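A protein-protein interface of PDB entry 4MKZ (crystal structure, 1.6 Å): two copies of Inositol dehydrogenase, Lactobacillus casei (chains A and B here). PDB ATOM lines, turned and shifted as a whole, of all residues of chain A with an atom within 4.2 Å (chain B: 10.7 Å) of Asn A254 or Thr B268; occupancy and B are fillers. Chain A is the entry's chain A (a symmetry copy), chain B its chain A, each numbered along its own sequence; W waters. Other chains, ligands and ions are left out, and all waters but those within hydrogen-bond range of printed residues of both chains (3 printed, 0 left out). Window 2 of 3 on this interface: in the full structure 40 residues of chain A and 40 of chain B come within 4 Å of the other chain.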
ATOM      1  N   ILE A 170      21.580 -22.776   6.199  1.00  0.00           N
ATOM      2  CA  ILE A 170      20.192 -23.124   6.508  1.00  0.00           C
ATOM      3  C   ILE A 170      20.092 -23.694   7.924  1.00  0.00           C
ATOM      4  O   ILE A 170      20.649 -24.747   8.225  1.00  0.00           O
ATOM      5  CB  ILE A 170      19.606 -24.128   5.495  1.00  0.00           C
ATOM      6  CG1 ILE A 170      19.962 -23.731   4.061  1.00  0.00           C
ATOM      7  CG2 ILE A 170      18.085 -24.220   5.654  1.00  0.00           C
ATOM      8  CD1 ILE A 170      19.407 -24.703   3.016  1.00  0.00           C
ATOM      9  N   ASP A 171      19.379 -22.983   8.790  1.00  0.00           N
ATOM     10  CA  ASP A 171      19.240 -23.394  10.184  1.00  0.00           C
ATOM     11  C   ASP A 171      18.264 -24.543  10.278  1.00  0.00           C
ATOM     12  O   ASP A 171      17.383 -24.676   9.437  1.00  0.00           O
ATOM     13  CB  ASP A 171      18.733 -22.225  11.027  1.00  0.00           C
ATOM     14  CG  ASP A 171      19.839 -21.493  11.738  1.00  0.00           C
ATOM     15  OD1 ASP A 171      20.983 -21.990  11.766  1.00  0.00           O
ATOM     16  OD2 ASP A 171      19.553 -20.418  12.291  1.00  0.00           O
ATOM     17  N   ALA A 173      15.159 -26.968  11.228  1.00  0.00           N
ATOM     18  CA  ALA A 173      13.730 -26.784  11.474  1.00  0.00           C
ATOM     19  C   ALA A 173      13.401 -26.768  12.965  1.00  0.00           C
ATOM     20  O   ALA A 173      12.399 -26.178  13.376  1.00  0.00           O
ATOM     21  CB  ALA A 173      12.933 -27.872  10.765  1.00  0.00           C
ATOM     22  N   MET A 176      12.586 -23.255  14.271  1.00  0.00           N
ATOM     23  CA  MET A 176      11.510 -22.458  13.675  1.00  0.00           C
ATOM     24  C   MET A 176      10.460 -21.979  14.676  1.00  0.00           C
ATOM     25  O   MET A 176      10.018 -20.832  14.615  1.00  0.00           O
ATOM     26  CB  MET A 176      10.816 -23.225  12.546  1.00  0.00           C
ATOM     27  CG  MET A 176      11.509 -23.147  11.200  1.00  0.00           C
ATOM     28  SD  MET A 176      11.855 -21.455  10.679  1.00  0.00           S
ATOM     29  CE  MET A 176      10.225 -20.714  10.764  1.00  0.00           C
ATOM     30  N   ARG A 221       6.905 -20.288   2.667  1.00  0.00           N
ATOM     31  CA  ARG A 221       6.011 -21.353   2.222  1.00  0.00           C
ATOM     32  C   ARG A 221       5.634 -22.307   3.336  1.00  0.00           C
ATOM     33  O   ARG A 221       4.538 -22.849   3.348  1.00  0.00           O
ATOM     34  CB  ARG A 221       6.668 -22.167   1.115  1.00  0.00           C
ATOM     35  CG  ARG A 221       5.741 -23.192   0.495  1.00  0.00           C
ATOM     36  CD  ARG A 221       5.187 -22.598  -0.752  1.00  0.00           C
ATOM     37  NE  ARG A 221       6.062 -22.864  -1.876  1.00  0.00           N
ATOM     38  CZ  ARG A 221       6.061 -22.173  -3.008  1.00  0.00           C
ATOM     39  NH1 ARG A 221       5.239 -21.143  -3.181  1.00  0.00           N
ATOM     40  NH2 ARG A 221       6.908 -22.503  -3.960  1.00  0.00           N
ATOM     41  N   ALA A 222       6.562 -22.549   4.250  1.00  0.00           N
ATOM     42  CA  ALA A 222       6.282 -23.433   5.371  1.00  0.00           C
ATOM     43  C   ALA A 222       5.657 -22.648   6.520  1.00  0.00           C
ATOM     44  O   ALA A 222       4.821 -23.167   7.261  1.00  0.00           O
ATOM     45  CB  ALA A 222       7.547 -24.140   5.828  1.00  0.00           C
ATOM     46  N   TYR A 223       6.075 -21.397   6.678  1.00  0.00           N
ATOM     47  CA  TYR A 223       5.537 -20.561   7.744  1.00  0.00           C
ATOM     48  C   TYR A 223       5.165 -19.162   7.230  1.00  0.00           C
ATOM     49  O   TYR A 223       5.939 -18.222   7.398  1.00  0.00           O
ATOM     50  CB  TYR A 223       6.555 -20.444   8.891  1.00  0.00           C
ATOM     51  CG  TYR A 223       6.947 -21.755   9.559  1.00  0.00           C
ATOM     52  CD1 TYR A 223       7.863 -22.620   8.964  1.00  0.00           C
ATOM     53  CD2 TYR A 223       6.437 -22.109  10.805  1.00  0.00           C
ATOM     54  CE1 TYR A 223       8.232 -23.811   9.569  1.00  0.00           C
ATOM     55  CE2 TYR A 223       6.807 -23.310  11.422  1.00  0.00           C
ATOM     56  CZ  TYR A 223       7.703 -24.152  10.797  1.00  0.00           C
ATOM     57  OH  TYR A 223       8.080 -25.343  11.398  1.00  0.00           O
ATOM     58  N   GLY A 252      18.192 -19.927   5.013  1.00  0.00           N
ATOM     59  CA  GLY A 252      16.951 -20.534   5.421  1.00  0.00           C
ATOM     60  C   GLY A 252      16.935 -20.841   6.890  1.00  0.00           C
ATOM     61  O   GLY A 252      17.962 -20.771   7.568  1.00  0.00           O
ATOM     62  N   ARG A 253      15.753 -21.172   7.390  1.00  0.00           N
ATOM     63  CA  ARG A 253      15.608 -21.421   8.816  1.00  0.00           C
ATOM     64  C   ARG A 253      14.909 -22.750   9.038  1.00  0.00           C
ATOM     65  O   ARG A 253      14.569 -23.097  10.166  1.00  0.00           O
ATOM     66  CB  ARG A 253      14.815 -20.282   9.461  1.00  0.00           C
ATOM     67  CG  ARG A 253      15.327 -18.885   9.145  1.00  0.00           C
ATOM     68  CD  ARG A 253      14.504 -17.834   9.867  1.00  0.00           C
ATOM     69  NE  ARG A 253      14.959 -16.466   9.611  1.00  0.00           N
ATOM     70  CZ  ARG A 253      15.961 -15.869  10.257  1.00  0.00           C
ATOM     71  NH1 ARG A 253      16.640 -16.523  11.187  1.00  0.00           N
ATOM     72  NH2 ARG A 253      16.291 -14.617   9.961  1.00  0.00           N
ATOM     73  N   ASN A 254      14.714 -23.498   7.954  1.00  0.00           N
ATOM     74  CA  ASN A 254      13.858 -24.679   7.981  1.00  0.00           C
ATOM     75  C   ASN A 254      14.452 -25.930   7.326  1.00  0.00           C
ATOM     76  O   ASN A 254      13.786 -26.597   6.531  1.00  0.00           O
ATOM     77  CB  ASN A 254      12.518 -24.338   7.318  1.00  0.00           C
ATOM     78  CG  ASN A 254      11.411 -25.285   7.716  1.00  0.00           C
ATOM     79  OD1 ASN A 254      11.413 -25.823   8.824  1.00  0.00           O
ATOM     80  ND2 ASN A 254      10.456 -25.498   6.810  1.00  0.00           N
ATOM     81  N   ALA A 255      15.698 -26.256   7.652  1.00  0.00           N
ATOM     82  CA  ALA A 255      16.314 -27.473   7.122  1.00  0.00           C
ATOM     83  C   ALA A 255      15.856 -28.697   7.912  1.00  0.00           C
ATOM     84  O   ALA A 255      15.980 -28.743   9.136  1.00  0.00           O
ATOM     85  CB  ALA A 255      17.837 -27.365   7.146  1.00  0.00           C
ATOM     86  N   ALA A 256      15.337 -29.698   7.216  1.00  0.00           N
ATOM     87  CA  ALA A 256      14.821 -30.876   7.900  1.00  0.00           C
ATOM     88  C   ALA A 256      15.931 -31.814   8.367  1.00  0.00           C
ATOM     89  O   ALA A 256      15.726 -32.613   9.278  1.00  0.00           O
ATOM     90  CB  ALA A 256      13.824 -31.619   7.009  1.00  0.00           C
ATOM     91  N   LEU B 153       9.092 -39.480  -5.351  1.00  0.00           N
ATOM     92  CA  LEU B 153       9.137 -38.965  -3.977  1.00  0.00           C
ATOM     93  C   LEU B 153       8.363 -37.655  -3.849  1.00  0.00           C
ATOM     94  O   LEU B 153       7.580 -37.476  -2.919  1.00  0.00           O
ATOM     95  CB  LEU B 153      10.582 -38.761  -3.489  1.00  0.00           C
ATOM     96  CG  LEU B 153      11.470 -40.002  -3.395  1.00  0.00           C
ATOM     97  CD1 LEU B 153      12.839 -39.613  -2.862  1.00  0.00           C
ATOM     98  CD2 LEU B 153      10.831 -41.056  -2.510  1.00  0.00           C
ATOM     99  N   VAL B 154       8.573 -36.740  -4.790  1.00  0.00           N
ATOM    100  CA  VAL B 154       7.866 -35.471  -4.775  1.00  0.00           C
ATOM    101  C   VAL B 154       6.357 -35.676  -4.918  1.00  0.00           C
ATOM    102  O   VAL B 154       5.581 -35.091  -4.162  1.00  0.00           O
ATOM    103  CB  VAL B 154       8.394 -34.515  -5.872  1.00  0.00           C
ATOM    104  CG1 VAL B 154       7.493 -33.297  -6.007  1.00  0.00           C
ATOM    105  CG2 VAL B 154       9.830 -34.086  -5.564  1.00  0.00           C
ATOM    106  N   GLY B 157       4.508 -36.734  -1.930  1.00  0.00           N
ATOM    107  CA  GLY B 157       4.483 -35.744  -0.865  1.00  0.00           C
ATOM    108  C   GLY B 157       5.630 -35.821   0.128  1.00  0.00           C
ATOM    109  O   GLY B 157       5.606 -35.145   1.158  1.00  0.00           O
ATOM    110  N   LYS B 158       6.654 -36.610  -0.191  1.00  0.00           N
ATOM    111  CA  LYS B 158       7.725 -36.903   0.761  1.00  0.00           C
ATOM    112  C   LYS B 158       8.617 -35.720   1.152  1.00  0.00           C
ATOM    113  O   LYS B 158       9.221 -35.743   2.216  1.00  0.00           O
ATOM    114  CB  LYS B 158       8.593 -38.072   0.281  1.00  0.00           C
ATOM    115  CG  LYS B 158       7.835 -39.344  -0.040  1.00  0.00           C
ATOM    116  CD  LYS B 158       6.947 -39.772   1.108  1.00  0.00           C
ATOM    117  CE  LYS B 158       6.360 -41.152   0.855  1.00  0.00           C
ATOM    118  NZ  LYS B 158       7.420 -42.180   0.700  1.00  0.00           N
ATOM    119  N   ILE B 159       8.721 -34.695   0.307  1.00  0.00           N
ATOM    120  CA  ILE B 159       9.462 -33.499   0.705  1.00  0.00           C
ATOM    121  C   ILE B 159       8.551 -32.284   0.845  1.00  0.00           C
ATOM    122  O   ILE B 159       9.021 -31.167   1.042  1.00  0.00           O
ATOM    123  CB  ILE B 159      10.641 -33.144  -0.238  1.00  0.00           C
ATOM    124  CG1 ILE B 159      10.125 -32.754  -1.618  1.00  0.00           C
ATOM    125  CG2 ILE B 159      11.644 -34.288  -0.323  1.00  0.00           C
ATOM    126  CD1 ILE B 159      11.175 -32.069  -2.468  1.00  0.00           C
ATOM    127  N   GLY B 160       7.245 -32.517   0.757  1.00  0.00           N
ATOM    128  CA  GLY B 160       6.274 -31.449   0.923  1.00  0.00           C
ATOM    129  C   GLY B 160       6.248 -30.584  -0.316  1.00  0.00           C
ATOM    130  O   GLY B 160       6.585 -31.043  -1.410  1.00  0.00           O
ATOM    131  N   ASP B 161       5.847 -29.329  -0.157  1.00  0.00           N
ATOM    132  CA  ASP B 161       5.838 -28.440  -1.304  1.00  0.00           C
ATOM    133  C   ASP B 161       7.257 -27.995  -1.614  1.00  0.00           C
ATOM    134  O   ASP B 161       8.076 -27.807  -0.715  1.00  0.00           O
ATOM    135  CB  ASP B 161       4.968 -27.220  -1.043  1.00  0.00           C
ATOM    136  CG  ASP B 161       4.784 -26.375  -2.282  1.00  0.00           C
ATOM    137  OD1 ASP B 161       4.697 -26.936  -3.401  1.00  0.00           O
ATOM    138  OD2 ASP B 161       4.740 -25.144  -2.138  1.00  0.00           O
ATOM    139  N   ILE B 162       7.542 -27.820  -2.896  1.00  0.00           N
ATOM    140  CA  ILE B 162       8.860 -27.393  -3.335  1.00  0.00           C
ATOM    141  C   ILE B 162       9.047 -25.902  -3.099  1.00  0.00           C
ATOM    142  O   ILE B 162       8.230 -25.095  -3.519  1.00  0.00           O
ATOM    143  CB  ILE B 162       9.037 -27.692  -4.833  1.00  0.00           C
ATOM    144  CG1 ILE B 162       9.019 -29.200  -5.060  1.00  0.00           C
ATOM    145  CG2 ILE B 162      10.322 -27.035  -5.357  1.00  0.00           C
ATOM    146  CD1 ILE B 162       8.971 -29.596  -6.534  1.00  0.00           C
ATOM    147  N   THR B 163      10.118 -25.533  -2.401  1.00  0.00           N
ATOM    148  CA  THR B 163      10.419 -24.130  -2.161  1.00  0.00           C
ATOM    149  C   THR B 163      11.505 -23.616  -3.112  1.00  0.00           C
ATOM    150  O   THR B 163      11.503 -22.464  -3.511  1.00  0.00           O
ATOM    151  CB  THR B 163      10.874 -23.892  -0.717  1.00  0.00           C
ATOM    152  OG1 THR B 163      12.179 -24.441  -0.544  1.00  0.00           O
ATOM    153  CG2 THR B 163       9.920 -24.545   0.266  1.00  0.00           C
ATOM    154  N   LEU B 164      12.436 -24.481  -3.482  1.00  0.00           N
ATOM    155  CA  LEU B 164      13.521 -24.054  -4.355  1.00  0.00           C
ATOM    156  C   LEU B 164      14.046 -25.223  -5.171  1.00  0.00           C
ATOM    157  O   LEU B 164      14.170 -26.341  -4.662  1.00  0.00           O
ATOM    158  CB  LEU B 164      14.658 -23.446  -3.512  1.00  0.00           C
ATOM    159  CG  LEU B 164      15.893 -22.899  -4.243  1.00  0.00           C
ATOM    160  CD1 LEU B 164      16.482 -21.736  -3.450  1.00  0.00           C
ATOM    161  CD2 LEU B 164      16.961 -23.972  -4.414  1.00  0.00           C
ATOM    162  N   ILE B 165      14.355 -24.962  -6.435  1.00  0.00           N
ATOM    163  CA  ILE B 165      15.052 -25.944  -7.245  1.00  0.00           C
ATOM    164  C   ILE B 165      16.335 -25.320  -7.768  1.00  0.00           C
ATOM    165  O   ILE B 165      16.321 -24.215  -8.289  1.00  0.00           O
ATOM    166  CB  ILE B 165      14.193 -26.448  -8.430  1.00  0.00           C
ATOM    167  CG1 ILE B 165      13.023 -27.269  -7.895  1.00  0.00           C
ATOM    168  CG2 ILE B 165      15.035 -27.296  -9.366  1.00  0.00           C
ATOM    169  CD1 ILE B 165      12.063 -27.737  -8.952  1.00  0.00           C
ATOM    170  N   LYS B 209       4.451 -25.518 -11.954  1.00  0.00           N
ATOM    171  CA  LYS B 209       4.322 -24.073 -11.899  1.00  0.00           C
ATOM    172  C   LYS B 209       5.099 -23.446 -13.054  1.00  0.00           C
ATOM    173  O   LYS B 209       5.913 -24.121 -13.694  1.00  0.00           O
ATOM    174  CB  LYS B 209       4.814 -23.567 -10.525  1.00  0.00           C
ATOM    175  CG  LYS B 209       4.294 -24.395  -9.322  1.00  0.00           C
ATOM    176  CD  LYS B 209       5.088 -24.151  -8.017  1.00  0.00           C
ATOM    177  CE  LYS B 209       4.676 -25.106  -6.885  1.00  0.00           C
ATOM    178  NZ  LYS B 209       5.481 -24.932  -5.628  1.00  0.00           N
ATOM    179  N   ASP B 243       4.285 -18.706  -7.758  1.00  0.00           N
ATOM    180  CA  ASP B 243       3.862 -18.719  -6.362  1.00  0.00           C
ATOM    181  C   ASP B 243       5.011 -18.306  -5.461  1.00  0.00           C
ATOM    182  O   ASP B 243       4.994 -18.564  -4.255  1.00  0.00           O
ATOM    183  CB  ASP B 243       3.369 -20.110  -5.964  1.00  0.00           C
ATOM    184  CG  ASP B 243       4.439 -21.171  -6.123  1.00  0.00           C
ATOM    185  OD1 ASP B 243       5.300 -21.010  -7.017  1.00  0.00           O
ATOM    186  OD2 ASP B 243       4.414 -22.164  -5.360  1.00  0.00           O
ATOM    187  N   THR B 245       7.951 -19.448  -5.663  1.00  0.00           N
ATOM    188  CA  THR B 245       8.923 -20.547  -5.670  1.00  0.00           C
ATOM    189  C   THR B 245      10.191 -20.000  -6.260  1.00  0.00           C
ATOM    190  O   THR B 245      10.157 -19.140  -7.142  1.00  0.00           O
ATOM    191  CB  THR B 245       8.473 -21.717  -6.597  1.00  0.00           C
ATOM    192  OG1 THR B 245       7.246 -22.254  -6.121  1.00  0.00           O
ATOM    193  CG2 THR B 245       9.516 -22.849  -6.650  1.00  0.00           C
ATOM    194  N   MET B 246      11.321 -20.523  -5.815  1.00  0.00           N
ATOM    195  CA  MET B 246      12.586 -20.008  -6.287  1.00  0.00           C
ATOM    196  C   MET B 246      13.298 -21.043  -7.117  1.00  0.00           C
ATOM    197  O   MET B 246      13.148 -22.240  -6.894  1.00  0.00           O
ATOM    198  CB  MET B 246      13.443 -19.630  -5.084  1.00  0.00           C
ATOM    199  CG  MET B 246      12.761 -18.614  -4.215  1.00  0.00           C
ATOM    200  SD  MET B 246      13.625 -18.273  -2.673  1.00  0.00           S
ATOM    201  CE  MET B 246      13.211 -19.708  -1.694  1.00  0.00           C
ATOM    202  N   ILE B 265      16.307 -30.327  -5.209  1.00  0.00           N
ATOM    203  CA  ILE B 265      14.965 -29.859  -4.903  1.00  0.00           C
ATOM    204  C   ILE B 265      14.861 -29.704  -3.395  1.00  0.00           C
ATOM    205  O   ILE B 265      15.065 -30.664  -2.659  1.00  0.00           O
ATOM    206  CB  ILE B 265      13.913 -30.884  -5.372  1.00  0.00           C
ATOM    207  CG1 ILE B 265      14.193 -31.291  -6.818  1.00  0.00           C
ATOM    208  CG2 ILE B 265      12.516 -30.286  -5.259  1.00  0.00           C
ATOM    209  CD1 ILE B 265      13.322 -32.394  -7.300  1.00  0.00           C
ATOM    210  N   ILE B 266      14.544 -28.496  -2.946  1.00  0.00           N
ATOM    211  CA  ILE B 266      14.325 -28.224  -1.532  1.00  0.00           C
ATOM    212  C   ILE B 266      12.827 -28.080  -1.279  1.00  0.00           C
ATOM    213  O   ILE B 266      12.142 -27.302  -1.945  1.00  0.00           O
ATOM    214  CB  ILE B 266      15.029 -26.934  -1.099  1.00  0.00           C
ATOM    215  CG1 ILE B 266      16.523 -27.006  -1.453  1.00  0.00           C
ATOM    216  CG2 ILE B 266      14.847 -26.712   0.405  1.00  0.00           C
ATOM    217  CD1 ILE B 266      17.333 -25.787  -1.001  1.00  0.00           C
ATOM    218  N   GLY B 267      12.316 -28.866  -0.344  1.00  0.00           N
ATOM    219  CA  GLY B 267      10.909 -28.820  -0.006  1.00  0.00           C
ATOM    220  C   GLY B 267      10.707 -28.468   1.454  1.00  0.00           C
ATOM    221  O   GLY B 267      11.670 -28.284   2.201  1.00  0.00           O
ATOM    222  N   THR B 268       9.451 -28.379   1.866  1.00  0.00           N
ATOM    223  CA  THR B 268       9.138 -27.982   3.234  1.00  0.00           C
ATOM    224  C   THR B 268       9.464 -29.083   4.233  1.00  0.00           C
ATOM    225  O   THR B 268       9.600 -28.813   5.420  1.00  0.00           O
ATOM    226  CB  THR B 268       7.655 -27.588   3.378  1.00  0.00           C
ATOM    227  OG1 THR B 268       6.828 -28.650   2.881  1.00  0.00           O
ATOM    228  CG2 THR B 268       7.378 -26.307   2.597  1.00  0.00           C
ATOM    229  N   LYS B 269       9.594 -30.318   3.756  1.00  0.00           N
ATOM    230  CA  LYS B 269       9.739 -31.465   4.650  1.00  0.00           C
ATOM    231  C   LYS B 269      11.040 -32.217   4.429  1.00  0.00           C
ATOM    232  O   LYS B 269      11.327 -33.205   5.115  1.00  0.00           O
ATOM    233  CB  LYS B 269       8.577 -32.432   4.454  1.00  0.00           C
ATOM    234  CG  LYS B 269       7.222 -31.799   4.678  1.00  0.00           C
ATOM    235  CD  LYS B 269       6.209 -32.853   5.067  1.00  0.00           C
ATOM    236  CE  LYS B 269       6.067 -33.889   3.981  1.00  0.00           C
ATOM    237  NZ  LYS B 269       5.926 -35.267   4.521  1.00  0.00           N
ATOM    238  N   GLY B 270      11.819 -31.761   3.458  1.00  0.00           N
ATOM    239  CA  GLY B 270      13.009 -32.488   3.070  1.00  0.00           C
ATOM    240  C   GLY B 270      13.664 -31.898   1.842  1.00  0.00           C
ATOM    241  O   GLY B 270      13.262 -30.845   1.336  1.00  0.00           O
ATOM    242  N   MET B 271      14.684 -32.588   1.355  1.00  0.00           N
ATOM    243  CA  MET B 271      15.513 -32.056   0.297  1.00  0.00           C
ATOM    244  C   MET B 271      16.073 -33.259  -0.431  1.00  0.00           C
ATOM    245  O   MET B 271      16.249 -34.322   0.162  1.00  0.00           O
ATOM    246  CB  MET B 271      16.636 -31.237   0.938  1.00  0.00           C
ATOM    247  CG  MET B 271      17.557 -30.511  -0.002  1.00  0.00           C
ATOM    248  SD  MET B 271      18.643 -29.439   0.974  1.00  0.00           S
ATOM    249  CE  MET B 271      19.718 -28.886  -0.349  1.00  0.00           C
ATOM    250  N   LEU B 272      16.313 -33.120  -1.724  1.00  0.00           N
ATOM    251  CA  LEU B 272      16.990 -34.193  -2.426  1.00  0.00           C
ATOM    252  C   LEU B 272      17.887 -33.610  -3.490  1.00  0.00           C
ATOM    253  O   LEU B 272      17.699 -32.472  -3.918  1.00  0.00           O
ATOM    254  CB  LEU B 272      16.007 -35.220  -3.004  1.00  0.00           C
ATOM    255  CG  LEU B 272      14.963 -34.707  -3.976  1.00  0.00           C
ATOM    256  CD1 LEU B 272      15.523 -34.662  -5.399  1.00  0.00           C
ATOM    257  CD2 LEU B 272      13.700 -35.588  -3.939  1.00  0.00           C
HETATM  258  O   HOH W   1       7.820 -27.233   7.436  1.00  0.00           O
HETATM  259  O   HOH W   2      11.512 -28.864   7.514  1.00  0.00           O
HETATM  260  O   HOH W   3      12.941 -27.994   4.331  1.00  0.00           O
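The side-chain carboxylate (OD2) of Asp B161 lies within salt-bridge range of the guanidinium group (NE) of Arg A221, at 2.6 Å. NH2 of Arg A221 lies close to OG1 of Thr B245, 2.2 Å away. The side-chain amino group (NZ) of Lys B209 lies close to the guanidinium group (NH2) of Arg A221, at 3.3 Å. NH1 of Arg A221 lies within salt-bridge range of OD2 of Asp B243. O of Ile B162 lies within hydrogen-bond range of NH2 of Arg A221, at 2.9 Å.
The backbone carbonyl oxygen of Ile B162 is in hydrogen-bond range of the side-chain amino group of Lys B209, at 3.5 Å. OD1 of Asp B243 sits at hydrogen-bond distance from OG1 of Thr B245 (2.5 Å). The side-chain amino group (NZ) of Lys B209 is in hydrogen-bond range of the side-chain hydroxyl (OG1) of Thr B245, 3.2 Å away. The side-chain carboxylate of Asp B243 is in salt-bridge range of the side-chain amino group of Lys B209, 3.0 Å away. OD1 of Asp B161 lies within salt-bridge range of NZ of Lys B209, at 3.1 Å. NZ of Lys B269 lies close to O of Gly B157.
Ala A222 touches Thr B268 (CB to CG2, 3.9 Å). Asn A254 touches Thr B268. CB of Ala A256 touches O of Lys B269, at 3.5 Å.
No residue of chain B comes within 4 Å of Ala A173. Printed residues of chain B within 4 Å of Arg A221: Asp B161, Ile B162, Lys B209, Asp B243 and Thr B245. Of chain B, only Thr B268 (3.9 Å) comes within 4 Å of Ala A222. No residue of chain B comes within 4 Å of Gly A252. Asn A254 touches just one residue of chain B: Thr B268 (3.7 Å). Printed residues of chain A within 4 Å of Asp B161: Arg A221 (2.6 Å). Printed residues of chain A within 4 Å of Lys B269: Ala A256 (3.5 Å). The nearest printed residue of chain B that does not touch Ala A256 is Gly B270 (4.1 Å).
Printed residues of chain A that touch a printed residue of chain B: Arg A221, Ala A222, Asn A254 and Ala A256. Hydrophobic or aromatic side chains of chain A that line the printed part of chain B: Ala A222 and Ala A256. Along chain A the printed residues that touch a printed residue of chain B span positions 221 to 256. Of the 23 printed residues of chain B, 7 touch a printed residue of chain A. Printed residues of chain B that touch a printed residue of chain A: Asp B161, Ile B162, Lys B209, Asp B243, Thr B245, Thr B268 and Lys B269. Among the printed residues, 8 pairs touch across the chains.
No position is printed for both chains.
Water W3 bridges the backbone carbonyl oxygen of Gly B267 and the backbone carbonyl oxygen of Asn A254. Water W2 bridges the backbone carbonyl oxygen (O) of Thr B268 (2.8 Å) and the side-chain amide oxygen (OD1) of Asn A254 (3.3 Å). Water W1 bridges the backbone carbonyl oxygen of Thr B268 and the side-chain amide nitrogen of Asn A254.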
